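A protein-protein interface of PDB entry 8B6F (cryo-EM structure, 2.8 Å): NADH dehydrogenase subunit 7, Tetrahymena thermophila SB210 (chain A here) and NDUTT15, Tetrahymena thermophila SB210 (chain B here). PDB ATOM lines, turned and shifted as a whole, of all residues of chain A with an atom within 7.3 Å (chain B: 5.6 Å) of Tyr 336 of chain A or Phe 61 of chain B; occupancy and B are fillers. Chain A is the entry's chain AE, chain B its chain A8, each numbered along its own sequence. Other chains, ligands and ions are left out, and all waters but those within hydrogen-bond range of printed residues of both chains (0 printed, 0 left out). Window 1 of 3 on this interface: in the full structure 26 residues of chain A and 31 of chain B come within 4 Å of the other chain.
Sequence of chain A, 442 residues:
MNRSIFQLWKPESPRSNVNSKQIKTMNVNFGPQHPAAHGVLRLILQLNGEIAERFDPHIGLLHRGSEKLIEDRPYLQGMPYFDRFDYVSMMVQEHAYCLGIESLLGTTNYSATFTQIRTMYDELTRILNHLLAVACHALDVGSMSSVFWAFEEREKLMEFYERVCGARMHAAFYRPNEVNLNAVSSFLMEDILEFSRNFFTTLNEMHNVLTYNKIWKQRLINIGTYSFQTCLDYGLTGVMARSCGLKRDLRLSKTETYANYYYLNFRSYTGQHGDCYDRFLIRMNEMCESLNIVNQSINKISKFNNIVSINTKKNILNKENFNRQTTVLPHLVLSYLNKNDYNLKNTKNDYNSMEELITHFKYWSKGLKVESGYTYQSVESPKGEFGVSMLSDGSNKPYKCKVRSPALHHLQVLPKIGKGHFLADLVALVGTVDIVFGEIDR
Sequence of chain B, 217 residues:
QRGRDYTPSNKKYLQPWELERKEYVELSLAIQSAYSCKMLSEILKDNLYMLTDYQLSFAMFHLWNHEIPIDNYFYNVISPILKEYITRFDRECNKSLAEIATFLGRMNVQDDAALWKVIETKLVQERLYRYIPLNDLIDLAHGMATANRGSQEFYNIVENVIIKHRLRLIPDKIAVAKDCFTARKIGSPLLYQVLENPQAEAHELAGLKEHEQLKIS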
ATOM      1  N   LYS A 300     -32.321 -10.664 -24.553  1.00  0.00           N
ATOM      2  CA  LYS A 300     -31.690 -10.437 -23.259  1.00  0.00           C
ATOM      3  C   LYS A 300     -32.402 -11.171 -22.130  1.00  0.00           C
ATOM      4  O   LYS A 300     -31.836 -11.306 -21.041  1.00  0.00           O
ATOM      5  CB  LYS A 300     -31.644  -8.938 -22.952  1.00  0.00           C
ATOM      6  CG  LYS A 300     -30.716  -8.142 -23.857  1.00  0.00           C
ATOM      7  CD  LYS A 300     -29.256  -8.411 -23.560  1.00  0.00           C
ATOM      8  CE  LYS A 300     -28.364  -7.701 -24.563  1.00  0.00           C
ATOM      9  NZ  LYS A 300     -26.932  -8.036 -24.359  1.00  0.00           N
ATOM     10  N   SER A 302     -33.918 -14.334 -22.597  1.00  0.00           N
ATOM     11  CA  SER A 302     -34.182 -15.642 -23.182  1.00  0.00           C
ATOM     12  C   SER A 302     -33.132 -16.642 -22.725  1.00  0.00           C
ATOM     13  O   SER A 302     -31.947 -16.310 -22.624  1.00  0.00           O
ATOM     14  CB  SER A 302     -34.183 -15.572 -24.711  1.00  0.00           C
ATOM     15  OG  SER A 302     -35.033 -14.541 -25.177  1.00  0.00           O
ATOM     16  N   LYS A 303     -33.571 -17.869 -22.456  1.00  0.00           N
ATOM     17  CA  LYS A 303     -32.681 -18.969 -22.085  1.00  0.00           C
ATOM     18  C   LYS A 303     -32.496 -19.841 -23.323  1.00  0.00           C
ATOM     19  O   LYS A 303     -33.264 -20.770 -23.572  1.00  0.00           O
ATOM     20  CB  LYS A 303     -33.249 -19.756 -20.912  1.00  0.00           C
ATOM     21  CG  LYS A 303     -32.287 -20.786 -20.341  1.00  0.00           C
ATOM     22  CD  LYS A 303     -32.888 -21.526 -19.156  1.00  0.00           C
ATOM     23  CE  LYS A 303     -33.950 -22.526 -19.584  1.00  0.00           C
ATOM     24  NZ  LYS A 303     -33.392 -23.602 -20.447  1.00  0.00           N
ATOM     25  N   PHE A 304     -31.463 -19.531 -24.110  1.00  0.00           N
ATOM     26  CA  PHE A 304     -31.244 -20.253 -25.361  1.00  0.00           C
ATOM     27  C   PHE A 304     -30.680 -21.647 -25.118  1.00  0.00           C
ATOM     28  O   PHE A 304     -31.089 -22.610 -25.778  1.00  0.00           O
ATOM     29  CB  PHE A 304     -30.312 -19.454 -26.270  1.00  0.00           C
ATOM     30  CG  PHE A 304     -30.861 -18.119 -26.674  1.00  0.00           C
ATOM     31  CD1 PHE A 304     -31.906 -18.032 -27.577  1.00  0.00           C
ATOM     32  CD2 PHE A 304     -30.324 -16.951 -26.160  1.00  0.00           C
ATOM     33  CE1 PHE A 304     -32.413 -16.806 -27.953  1.00  0.00           C
ATOM     34  CE2 PHE A 304     -30.828 -15.720 -26.531  1.00  0.00           C
ATOM     35  CZ  PHE A 304     -31.873 -15.649 -27.430  1.00  0.00           C
ATOM     36  N   ASN A 305     -29.744 -21.778 -24.185  1.00  0.00           N
ATOM     37  CA  ASN A 305     -29.073 -23.048 -23.965  1.00  0.00           C
ATOM     38  C   ASN A 305     -29.901 -23.938 -23.040  1.00  0.00           C
ATOM     39  O   ASN A 305     -30.879 -23.508 -22.425  1.00  0.00           O
ATOM     40  CB  ASN A 305     -27.677 -22.814 -23.389  1.00  0.00           C
ATOM     41  CG  ASN A 305     -26.737 -23.972 -23.645  1.00  0.00           C
ATOM     42  OD1 ASN A 305     -27.038 -24.868 -24.432  1.00  0.00           O
ATOM     43  ND2 ASN A 305     -25.584 -23.954 -22.989  1.00  0.00           N
ATOM     44  N   HIS A 331     -39.034 -12.817 -16.347  1.00  0.00           N
ATOM     45  CA  HIS A 331     -38.567 -12.634 -14.979  1.00  0.00           C
ATOM     46  C   HIS A 331     -37.204 -13.267 -14.737  1.00  0.00           C
ATOM     47  O   HIS A 331     -36.774 -13.365 -13.584  1.00  0.00           O
ATOM     48  CB  HIS A 331     -39.588 -13.211 -13.999  1.00  0.00           C
ATOM     49  CG  HIS A 331     -40.964 -12.647 -14.164  1.00  0.00           C
ATOM     50  ND1 HIS A 331     -42.091 -13.280 -13.686  1.00  0.00           N
ATOM     51  CD2 HIS A 331     -41.396 -11.509 -14.757  1.00  0.00           C
ATOM     52  CE1 HIS A 331     -43.158 -12.557 -13.977  1.00  0.00           C
ATOM     53  NE2 HIS A 331     -42.763 -11.477 -14.627  1.00  0.00           N
ATOM     54  N   LEU A 332     -36.524 -13.703 -15.797  1.00  0.00           N
ATOM     55  CA  LEU A 332     -35.249 -14.395 -15.644  1.00  0.00           C
ATOM     56  C   LEU A 332     -34.232 -13.525 -14.913  1.00  0.00           C
ATOM     57  O   LEU A 332     -33.762 -13.873 -13.826  1.00  0.00           O
ATOM     58  CB  LEU A 332     -34.727 -14.802 -17.022  1.00  0.00           C
ATOM     59  CG  LEU A 332     -33.370 -15.501 -17.079  1.00  0.00           C
ATOM     60  CD1 LEU A 332     -33.393 -16.772 -16.261  1.00  0.00           C
ATOM     61  CD2 LEU A 332     -32.997 -15.795 -18.519  1.00  0.00           C
ATOM     62  N   VAL A 333     -33.878 -12.384 -15.506  1.00  0.00           N
ATOM     63  CA  VAL A 333     -32.823 -11.547 -14.942  1.00  0.00           C
ATOM     64  C   VAL A 333     -33.252 -10.969 -13.600  1.00  0.00           C
ATOM     65  O   VAL A 333     -32.456 -10.900 -12.658  1.00  0.00           O
ATOM     66  CB  VAL A 333     -32.435 -10.438 -15.938  1.00  0.00           C
ATOM     67  CG1 VAL A 333     -31.321  -9.570 -15.368  1.00  0.00           C
ATOM     68  CG2 VAL A 333     -32.013 -11.040 -17.269  1.00  0.00           C
ATOM     69  N   LEU A 334     -34.509 -10.539 -13.492  1.00  0.00           N
ATOM     70  CA  LEU A 334     -34.984  -9.959 -12.240  1.00  0.00           C
ATOM     71  C   LEU A 334     -34.887 -10.964 -11.101  1.00  0.00           C
ATOM     72  O   LEU A 334     -34.399 -10.643 -10.013  1.00  0.00           O
ATOM     73  CB  LEU A 334     -36.422  -9.465 -12.405  1.00  0.00           C
ATOM     74  CG  LEU A 334     -37.019  -8.728 -11.204  1.00  0.00           C
ATOM     75  CD1 LEU A 334     -36.279  -7.430 -10.942  1.00  0.00           C
ATOM     76  CD2 LEU A 334     -38.496  -8.465 -11.423  1.00  0.00           C
ATOM     77  N   SER A 335     -35.349 -12.192 -11.335  1.00  0.00           N
ATOM     78  CA  SER A 335     -35.255 -13.222 -10.308  1.00  0.00           C
ATOM     79  C   SER A 335     -33.804 -13.555  -9.993  1.00  0.00           C
ATOM     80  O   SER A 335     -33.444 -13.762  -8.828  1.00  0.00           O
ATOM     81  CB  SER A 335     -35.996 -14.479 -10.762  1.00  0.00           C
ATOM     82  OG  SER A 335     -37.332 -14.181 -11.122  1.00  0.00           O
ATOM     83  N   TYR A 336     -32.954 -13.618 -11.019  1.00  0.00           N
ATOM     84  CA  TYR A 336     -31.562 -13.994 -10.802  1.00  0.00           C
ATOM     85  C   TYR A 336     -30.835 -12.969  -9.941  1.00  0.00           C
ATOM     86  O   TYR A 336     -30.068 -13.337  -9.044  1.00  0.00           O
ATOM     87  CB  TYR A 336     -30.857 -14.157 -12.149  1.00  0.00           C
ATOM     88  CG  TYR A 336     -29.599 -14.991 -12.091  1.00  0.00           C
ATOM     89  CD1 TYR A 336     -28.430 -14.485 -11.540  1.00  0.00           C
ATOM     90  CD2 TYR A 336     -29.578 -16.282 -12.601  1.00  0.00           C
ATOM     91  CE1 TYR A 336     -27.278 -15.244 -11.490  1.00  0.00           C
ATOM     92  CE2 TYR A 336     -28.432 -17.049 -12.556  1.00  0.00           C
ATOM     93  CZ  TYR A 336     -27.285 -16.524 -12.001  1.00  0.00           C
ATOM     94  OH  TYR A 336     -26.141 -17.284 -11.953  1.00  0.00           O
ATOM     95  N   LEU A 337     -31.062 -11.681 -10.193  1.00  0.00           N
ATOM     96  CA  LEU A 337     -30.312 -10.628  -9.513  1.00  0.00           C
ATOM     97  C   LEU A 337     -31.008 -10.163  -8.235  1.00  0.00           C
ATOM     98  O   LEU A 337     -30.442 -10.264  -7.143  1.00  0.00           O
ATOM     99  CB  LEU A 337     -30.090  -9.449 -10.468  1.00  0.00           C
ATOM    100  CG  LEU A 337     -29.259  -9.753 -11.718  1.00  0.00           C
ATOM    101  CD1 LEU A 337     -29.158  -8.524 -12.600  1.00  0.00           C
ATOM    102  CD2 LEU A 337     -27.873 -10.255 -11.355  1.00  0.00           C
ATOM    103  N   ASN A 338     -32.232  -9.652  -8.354  1.00  0.00           N
ATOM    104  CA  ASN A 338     -32.974  -9.158  -7.195  1.00  0.00           C
ATOM    105  C   ASN A 338     -33.917 -10.247  -6.689  1.00  0.00           C
ATOM    106  O   ASN A 338     -35.133 -10.208  -6.874  1.00  0.00           O
ATOM    107  CB  ASN A 338     -33.733  -7.884  -7.554  1.00  0.00           C
ATOM    108  CG  ASN A 338     -32.812  -6.709  -7.805  1.00  0.00           C
ATOM    109  OD1 ASN A 338     -32.344  -6.499  -8.921  1.00  0.00           O
ATOM    110  ND2 ASN A 338     -32.548  -5.933  -6.759  1.00  0.00           N
ATOM    111  N   LYS A 339     -33.319 -11.238  -6.029  1.00  0.00           N
ATOM    112  CA  LYS A 339     -34.099 -12.368  -5.539  1.00  0.00           C
ATOM    113  C   LYS A 339     -34.955 -11.967  -4.345  1.00  0.00           C
ATOM    114  O   LYS A 339     -36.139 -12.313  -4.272  1.00  0.00           O
ATOM    115  CB  LYS A 339     -33.170 -13.526  -5.175  1.00  0.00           C
ATOM    116  CG  LYS A 339     -33.886 -14.843  -4.909  1.00  0.00           C
ATOM    117  CD  LYS A 339     -34.544 -15.382  -6.171  1.00  0.00           C
ATOM    118  CE  LYS A 339     -35.165 -16.749  -5.934  1.00  0.00           C
ATOM    119  NZ  LYS A 339     -35.815 -17.282  -7.165  1.00  0.00           N
ATOM    120  N   TYR A 342     -37.829  -9.679  -5.467  1.00  0.00           N
ATOM    121  CA  TYR A 342     -38.820 -10.456  -6.201  1.00  0.00           C
ATOM    122  C   TYR A 342     -39.651 -11.315  -5.256  1.00  0.00           C
ATOM    123  O   TYR A 342     -40.876 -11.392  -5.391  1.00  0.00           O
ATOM    124  CB  TYR A 342     -38.116 -11.320  -7.249  1.00  0.00           C
ATOM    125  CG  TYR A 342     -39.045 -12.074  -8.170  1.00  0.00           C
ATOM    126  CD1 TYR A 342     -39.618 -11.450  -9.269  1.00  0.00           C
ATOM    127  CD2 TYR A 342     -39.332 -13.413  -7.952  1.00  0.00           C
ATOM    128  CE1 TYR A 342     -40.461 -12.137 -10.120  1.00  0.00           C
ATOM    129  CE2 TYR A 342     -40.172 -14.109  -8.796  1.00  0.00           C
ATOM    130  CZ  TYR A 342     -40.734 -13.465  -9.878  1.00  0.00           C
ATOM    131  OH  TYR A 342     -41.574 -14.154 -10.722  1.00  0.00           O
ATOM    132  N   TYR B  54     -23.822 -12.081  -6.735  1.00  0.00           N
ATOM    133  CA  TYR B  54     -24.956 -12.255  -7.636  1.00  0.00           C
ATOM    134  C   TYR B  54     -24.568 -11.924  -9.069  1.00  0.00           C
ATOM    135  O   TYR B  54     -24.878 -12.674 -10.001  1.00  0.00           O
ATOM    136  CB  TYR B  54     -26.122 -11.370  -7.195  1.00  0.00           C
ATOM    137  CG  TYR B  54     -26.701 -11.716  -5.847  1.00  0.00           C
ATOM    138  CD1 TYR B  54     -27.439 -12.876  -5.666  1.00  0.00           C
ATOM    139  CD2 TYR B  54     -26.533 -10.870  -4.763  1.00  0.00           C
ATOM    140  CE1 TYR B  54     -27.981 -13.193  -4.439  1.00  0.00           C
ATOM    141  CE2 TYR B  54     -27.069 -11.176  -3.531  1.00  0.00           C
ATOM    142  CZ  TYR B  54     -27.792 -12.338  -3.375  1.00  0.00           C
ATOM    143  OH  TYR B  54     -28.329 -12.649  -2.149  1.00  0.00           O
ATOM    144  N   LEU B  56     -21.545 -11.800 -10.401  1.00  0.00           N
ATOM    145  CA  LEU B  56     -20.557 -12.743 -10.913  1.00  0.00           C
ATOM    146  C   LEU B  56     -21.222 -14.034 -11.374  1.00  0.00           C
ATOM    147  O   LEU B  56     -20.901 -14.555 -12.447  1.00  0.00           O
ATOM    148  CB  LEU B  56     -19.503 -13.023  -9.842  1.00  0.00           C
ATOM    149  CG  LEU B  56     -18.238 -13.773 -10.266  1.00  0.00           C
ATOM    150  CD1 LEU B  56     -17.503 -13.057 -11.389  1.00  0.00           C
ATOM    151  CD2 LEU B  56     -17.326 -13.947  -9.064  1.00  0.00           C
ATOM    152  N   SER B  57     -22.151 -14.565 -10.576  1.00  0.00           N
ATOM    153  CA  SER B  57     -22.886 -15.754 -10.992  1.00  0.00           C
ATOM    154  C   SER B  57     -23.705 -15.475 -12.246  1.00  0.00           C
ATOM    155  O   SER B  57     -23.828 -16.338 -13.121  1.00  0.00           O
ATOM    156  CB  SER B  57     -23.787 -16.244  -9.858  1.00  0.00           C
ATOM    157  OG  SER B  57     -24.737 -15.259  -9.496  1.00  0.00           O
ATOM    158  N   PHE B  58     -24.273 -14.273 -12.346  1.00  0.00           N
ATOM    159  CA  PHE B  58     -25.032 -13.909 -13.537  1.00  0.00           C
ATOM    160  C   PHE B  58     -24.129 -13.820 -14.759  1.00  0.00           C
ATOM    161  O   PHE B  58     -24.534 -14.199 -15.865  1.00  0.00           O
ATOM    162  CB  PHE B  58     -25.762 -12.585 -13.319  1.00  0.00           C
ATOM    163  CG  PHE B  58     -26.623 -12.177 -14.478  1.00  0.00           C
ATOM    164  CD1 PHE B  58     -27.795 -12.860 -14.757  1.00  0.00           C
ATOM    165  CD2 PHE B  58     -26.263 -11.111 -15.284  1.00  0.00           C
ATOM    166  CE1 PHE B  58     -28.589 -12.492 -15.822  1.00  0.00           C
ATOM    167  CE2 PHE B  58     -27.053 -10.736 -16.349  1.00  0.00           C
ATOM    168  CZ  PHE B  58     -28.219 -11.427 -16.618  1.00  0.00           C
ATOM    169  N   ALA B  59     -22.903 -13.329 -14.581  1.00  0.00           N
ATOM    170  CA  ALA B  59     -21.958 -13.306 -15.690  1.00  0.00           C
ATOM    171  C   ALA B  59     -21.636 -14.718 -16.158  1.00  0.00           C
ATOM    172  O   ALA B  59     -21.574 -14.980 -17.364  1.00  0.00           O
ATOM    173  CB  ALA B  59     -20.681 -12.576 -15.276  1.00  0.00           C
ATOM    174  N   MET B  60     -21.426 -15.641 -15.220  1.00  0.00           N
ATOM    175  CA  MET B  60     -21.198 -17.031 -15.597  1.00  0.00           C
ATOM    176  C   MET B  60     -22.402 -17.596 -16.340  1.00  0.00           C
ATOM    177  O   MET B  60     -22.248 -18.302 -17.342  1.00  0.00           O
ATOM    178  CB  MET B  60     -20.892 -17.867 -14.356  1.00  0.00           C
ATOM    179  CG  MET B  60     -19.617 -17.464 -13.633  1.00  0.00           C
ATOM    180  SD  MET B  60     -18.137 -17.602 -14.654  1.00  0.00           S
ATOM    181  CE  MET B  60     -17.979 -15.926 -15.270  1.00  0.00           C
ATOM    182  N   PHE B  61     -23.611 -17.294 -15.863  1.00  0.00           N
ATOM    183  CA  PHE B  61     -24.812 -17.767 -16.543  1.00  0.00           C
ATOM    184  C   PHE B  61     -24.901 -17.200 -17.953  1.00  0.00           C
ATOM    185  O   PHE B  61     -25.279 -17.907 -18.893  1.00  0.00           O
ATOM    186  CB  PHE B  61     -26.060 -17.389 -15.749  1.00  0.00           C
ATOM    187  CG  PHE B  61     -27.317 -17.405 -16.568  1.00  0.00           C
ATOM    188  CD1 PHE B  61     -27.896 -18.602 -16.947  1.00  0.00           C
ATOM    189  CD2 PHE B  61     -27.916 -16.222 -16.967  1.00  0.00           C
ATOM    190  CE1 PHE B  61     -29.048 -18.623 -17.704  1.00  0.00           C
ATOM    191  CE2 PHE B  61     -29.069 -16.237 -17.726  1.00  0.00           C
ATOM    192  CZ  PHE B  61     -29.635 -17.440 -18.094  1.00  0.00           C
ATOM    193  N   HIS B  62     -24.563 -15.921 -18.117  1.00  0.00           N
ATOM    194  CA  HIS B  62     -24.595 -15.313 -19.442  1.00  0.00           C
ATOM    195  C   HIS B  62     -23.602 -15.988 -20.378  1.00  0.00           C
ATOM    196  O   HIS B  62     -23.929 -16.278 -21.534  1.00  0.00           O
ATOM    197  CB  HIS B  62     -24.303 -13.815 -19.327  1.00  0.00           C
ATOM    198  CG  HIS B  62     -24.121 -13.130 -20.643  1.00  0.00           C
ATOM    199  ND1 HIS B  62     -25.169 -12.871 -21.500  1.00  0.00           N
ATOM    200  CD2 HIS B  62     -23.012 -12.640 -21.246  1.00  0.00           C
ATOM    201  CE1 HIS B  62     -24.714 -12.256 -22.575  1.00  0.00           C
ATOM    202  NE2 HIS B  62     -23.408 -12.104 -22.447  1.00  0.00           N
ATOM    203  N   LEU B  63     -22.383 -16.244 -19.901  1.00  0.00           N
ATOM    204  CA  LEU B  63     -21.402 -16.941 -20.728  1.00  0.00           C
ATOM    205  C   LEU B  63     -21.921 -18.308 -21.155  1.00  0.00           C
ATOM    206  O   LEU B  63     -21.824 -18.685 -22.328  1.00  0.00           O
ATOM    207  CB  LEU B  63     -20.085 -17.089 -19.967  1.00  0.00           C
ATOM    208  CG  LEU B  63     -19.289 -15.818 -19.670  1.00  0.00           C
ATOM    209  CD1 LEU B  63     -18.040 -16.172 -18.885  1.00  0.00           C
ATOM    210  CD2 LEU B  63     -18.925 -15.081 -20.947  1.00  0.00           C
ATOM    211  N   TRP B  64     -22.474 -19.069 -20.209  1.00  0.00           N
ATOM    212  CA  TRP B  64     -23.008 -20.387 -20.536  1.00  0.00           C
ATOM    213  C   TRP B  64     -24.170 -20.282 -21.512  1.00  0.00           C
ATOM    214  O   TRP B  64     -24.260 -21.060 -22.469  1.00  0.00           O
ATOM    215  CB  TRP B  64     -23.453 -21.111 -19.268  1.00  0.00           C
ATOM    216  CG  TRP B  64     -24.296 -22.322 -19.547  1.00  0.00           C
ATOM    217  CD1 TRP B  64     -23.848 -23.571 -19.856  1.00  0.00           C
ATOM    218  CD2 TRP B  64     -25.728 -22.396 -19.548  1.00  0.00           C
ATOM    219  NE1 TRP B  64     -24.910 -24.419 -20.047  1.00  0.00           N
ATOM    220  CE2 TRP B  64     -26.075 -23.723 -19.865  1.00  0.00           C
ATOM    221  CE3 TRP B  64     -26.747 -21.470 -19.311  1.00  0.00           C
ATOM    222  CZ2 TRP B  64     -27.398 -24.147 -19.949  1.00  0.00           C
ATOM    223  CZ3 TRP B  64     -28.062 -21.893 -19.396  1.00  0.00           C
ATOM    224  CH2 TRP B  64     -28.376 -23.221 -19.713  1.00  0.00           C
ATOM    225  N   ASN B  65     -25.072 -19.325 -21.287  1.00  0.00           N
ATOM    226  CA  ASN B  65     -26.273 -19.236 -22.109  1.00  0.00           C
ATOM    227  C   ASN B  65     -25.931 -18.910 -23.556  1.00  0.00           C
ATOM    228  O   ASN B  65     -26.505 -19.496 -24.482  1.00  0.00           O
ATOM    229  CB  ASN B  65     -27.212 -18.180 -21.529  1.00  0.00           C
ATOM    230  CG  ASN B  65     -28.563 -18.167 -22.206  1.00  0.00           C
ATOM    231  OD1 ASN B  65     -28.972 -19.149 -22.819  1.00  0.00           O
ATOM    232  ND2 ASN B  65     -29.268 -17.047 -22.096  1.00  0.00           N
ATOM    233  N   HIS B  66     -25.005 -17.983 -23.774  1.00  0.00           N
ATOM    234  CA  HIS B  66     -24.616 -17.587 -25.120  1.00  0.00           C
ATOM    235  C   HIS B  66     -23.426 -18.374 -25.651  1.00  0.00           C
ATOM    236  O   HIS B  66     -22.953 -18.082 -26.753  1.00  0.00           O
ATOM    237  CB  HIS B  66     -24.306 -16.089 -25.151  1.00  0.00           C
ATOM    238  CG  HIS B  66     -25.524 -15.228 -25.036  1.00  0.00           C
ATOM    239  ND1 HIS B  66     -26.155 -14.682 -26.134  1.00  0.00           N
ATOM    240  CD2 HIS B  66     -26.239 -14.834 -23.957  1.00  0.00           C
ATOM    241  CE1 HIS B  66     -27.202 -13.985 -25.734  1.00  0.00           C
ATOM    242  NE2 HIS B  66     -27.276 -14.060 -24.418  1.00  0.00           N
ATOM    243  N   LYS B  95     -26.772 -19.762  -3.026  1.00  0.00           N
ATOM    244  CA  LYS B  95     -27.283 -19.543  -4.374  1.00  0.00           C
ATOM    245  C   LYS B  95     -26.144 -19.254  -5.344  1.00  0.00           C
ATOM    246  O   LYS B  95     -26.050 -19.869  -6.411  1.00  0.00           O
ATOM    247  CB  LYS B  95     -28.292 -18.394  -4.366  1.00  0.00           C
ATOM    248  CG  LYS B  95     -28.885 -18.070  -5.730  1.00  0.00           C
ATOM    249  CD  LYS B  95     -29.810 -16.863  -5.653  1.00  0.00           C
ATOM    250  CE  LYS B  95     -30.421 -16.543  -7.006  1.00  0.00           C
ATOM    251  NZ  LYS B  95     -31.263 -17.663  -7.516  1.00  0.00           N
ATOM    252  N   GLU B  99     -24.927 -21.739  -8.399  1.00  0.00           N
ATOM    253  CA  GLU B  99     -25.021 -21.240  -9.767  1.00  0.00           C
ATOM    254  C   GLU B  99     -23.658 -21.242 -10.447  1.00  0.00           C
ATOM    255  O   GLU B  99     -23.513 -21.740 -11.568  1.00  0.00           O
ATOM    256  CB  GLU B  99     -25.625 -19.836  -9.771  1.00  0.00           C
ATOM    257  CG  GLU B  99     -27.092 -19.798  -9.372  1.00  0.00           C
ATOM    258  CD  GLU B  99     -27.616 -18.385  -9.200  1.00  0.00           C
ATOM    259  OE1 GLU B  99     -26.792 -17.451  -9.106  1.00  0.00           O
ATOM    260  OE2 GLU B  99     -28.851 -18.206  -9.160  1.00  0.00           O
ATOM    261  N   ILE B 100     -22.642 -20.699  -9.777  1.00  0.00           N
ATOM    262  CA  ILE B 100     -21.318 -20.609 -10.391  1.00  0.00           C
ATOM    263  C   ILE B 100     -20.787 -22.001 -10.699  1.00  0.00           C
ATOM    264  O   ILE B 100     -20.296 -22.271 -11.801  1.00  0.00           O
ATOM    265  CB  ILE B 100     -20.357 -19.821  -9.482  1.00  0.00           C
ATOM    266  CG1 ILE B 100     -20.794 -18.357  -9.408  1.00  0.00           C
ATOM    267  CG2 ILE B 100     -18.920 -19.929  -9.987  1.00  0.00           C
ATOM    268  CD1 ILE B 100     -20.039 -17.535  -8.387  1.00  0.00           C
ATOM    269  N   PHE B 103     -22.788 -23.708 -13.640  1.00  0.00           N
ATOM    270  CA  PHE B 103     -22.547 -23.161 -14.971  1.00  0.00           C
ATOM    271  C   PHE B 103     -21.110 -23.379 -15.421  1.00  0.00           C
ATOM    272  O   PHE B 103     -20.862 -23.563 -16.617  1.00  0.00           O
ATOM    273  CB  PHE B 103     -22.921 -21.681 -15.002  1.00  0.00           C
ATOM    274  CG  PHE B 103     -24.399 -21.439 -14.892  1.00  0.00           C
ATOM    275  CD1 PHE B 103     -25.266 -21.932 -15.853  1.00  0.00           C
ATOM    276  CD2 PHE B 103     -24.924 -20.727 -13.829  1.00  0.00           C
ATOM    277  CE1 PHE B 103     -26.625 -21.719 -15.756  1.00  0.00           C
ATOM    278  CE2 PHE B 103     -26.283 -20.511 -13.725  1.00  0.00           C
ATOM    279  CZ  PHE B 103     -27.135 -21.009 -14.690  1.00  0.00           C
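The side-chain amide nitrogen (ND2) of Asn 305 of chain A sits close to the indole nitrogen (NE1) of Trp 64 of chain B (3.1 Å). The backbone NH (N) of Asn 305 of chain A is in hydrogen-bond range of the side-chain amide oxygen (OD1) of Asn 65 of chain B (3.1 Å). The side-chain amide oxygen (OD1) of Asn 65 of chain B is in hydrogen-bond range of the backbone NH (N) of Phe 304 of chain A (2.8 Å). OH of Tyr 336 of chain A lies within hydrogen-bond range of OE1 of Glu 99 of chain B (2.9 Å). OH of Tyr 336 of chain A is in hydrogen-bond range of O of Ser 57 of chain B, 2.8 Å away. The backbone carbonyl oxygen (O) of Ser 302 of chain A lies within hydrogen-bond range of the side-chain amide nitrogen (ND2) of Asn 65 of chain B.
Printed residues of chain A that touch a printed residue of chain B: Ser 302, Lys 303, Phe 304, Asn 305, Leu 332, Val 333, Tyr 336 and Leu 337. Hydrophobic or aromatic side chains of chain A within 4 Å of the printed part of chain B: Phe 304, Leu 332, Val 333, Tyr 336 and Leu 337. Along chain B the printed residues that touch a printed residue of chain A span positions 54 to 103.
The side-chain carboxylate of Glu 99 of chain B lies within hydrogen-bond range of the side-chain hydroxyl of Ser 57 of chain B, at 3.0 Å. The side-chain hydroxyl of Ser 57 of chain B sits at hydrogen-bond distance from the backbone carbonyl oxygen of Tyr 54 of chain B (2.6 Å). The side-chain carboxylate (OE2) of Glu 99 of chain B is in salt-bridge range of the side-chain amino group (NZ) of Lys 95 of chain B (3.0 Å). NZ of Lys 303 of chain A lies within hydrogen-bond range of O of Asn 305 of chain A, 3.2 Å away.
Of chain B, only Tyr 54, Ser 57, Phe 58, Phe 61, Lys 95, Glu 99 and Phe 103 come within 4 Å of Tyr 336 of chain A. Phe 61 of chain B touches just these residues of chain A: Leu 332 (3.8 Å) and Tyr 336 (3.8 Å). Of the printed residues of chain A, Glu 99 of chain B touches Tyr 336. Printed residues of chain B within 4 Å of Asn 305 of chain A: Trp 64 and Asn 65. Leu 56 of chain B touches none of the printed residues of chain A. Lys 300 of chain A touches none of the printed residues of chain B. The nearest residue of chain B that does not touch Tyr 336 of chain A is Ile 100 of chain B (5.4 Å). The nearest printed residue of chain A that does not touch Trp 64 of chain B is Lys 303 of chain A (4.5 Å).
Among the printed residues, pairs that only touch across the chains: Tyr 336 of chain A with Phe 58 of chain B (3.3 Å), Lys 303 of chain A with Asn 65 of chain B (3.6 Å), Tyr 336 of chain A with Phe 103 of chain B (3.7 Å), Leu 337 of chain A with Phe 58 of chain B (3.7 Å), Leu 332 of chain A with Phe 61 of chain B (3.8 Å), Tyr 336 of chain A with Phe 61 of chain B (3.8 Å), Tyr 336 of chain A with Lys 95 of chain B (3.8 Å), Tyr 336 of chain A with Tyr 54 of chain B (3.8 Å) and Val 333 of chain A with Phe 58 of chain B (3.8 Å).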
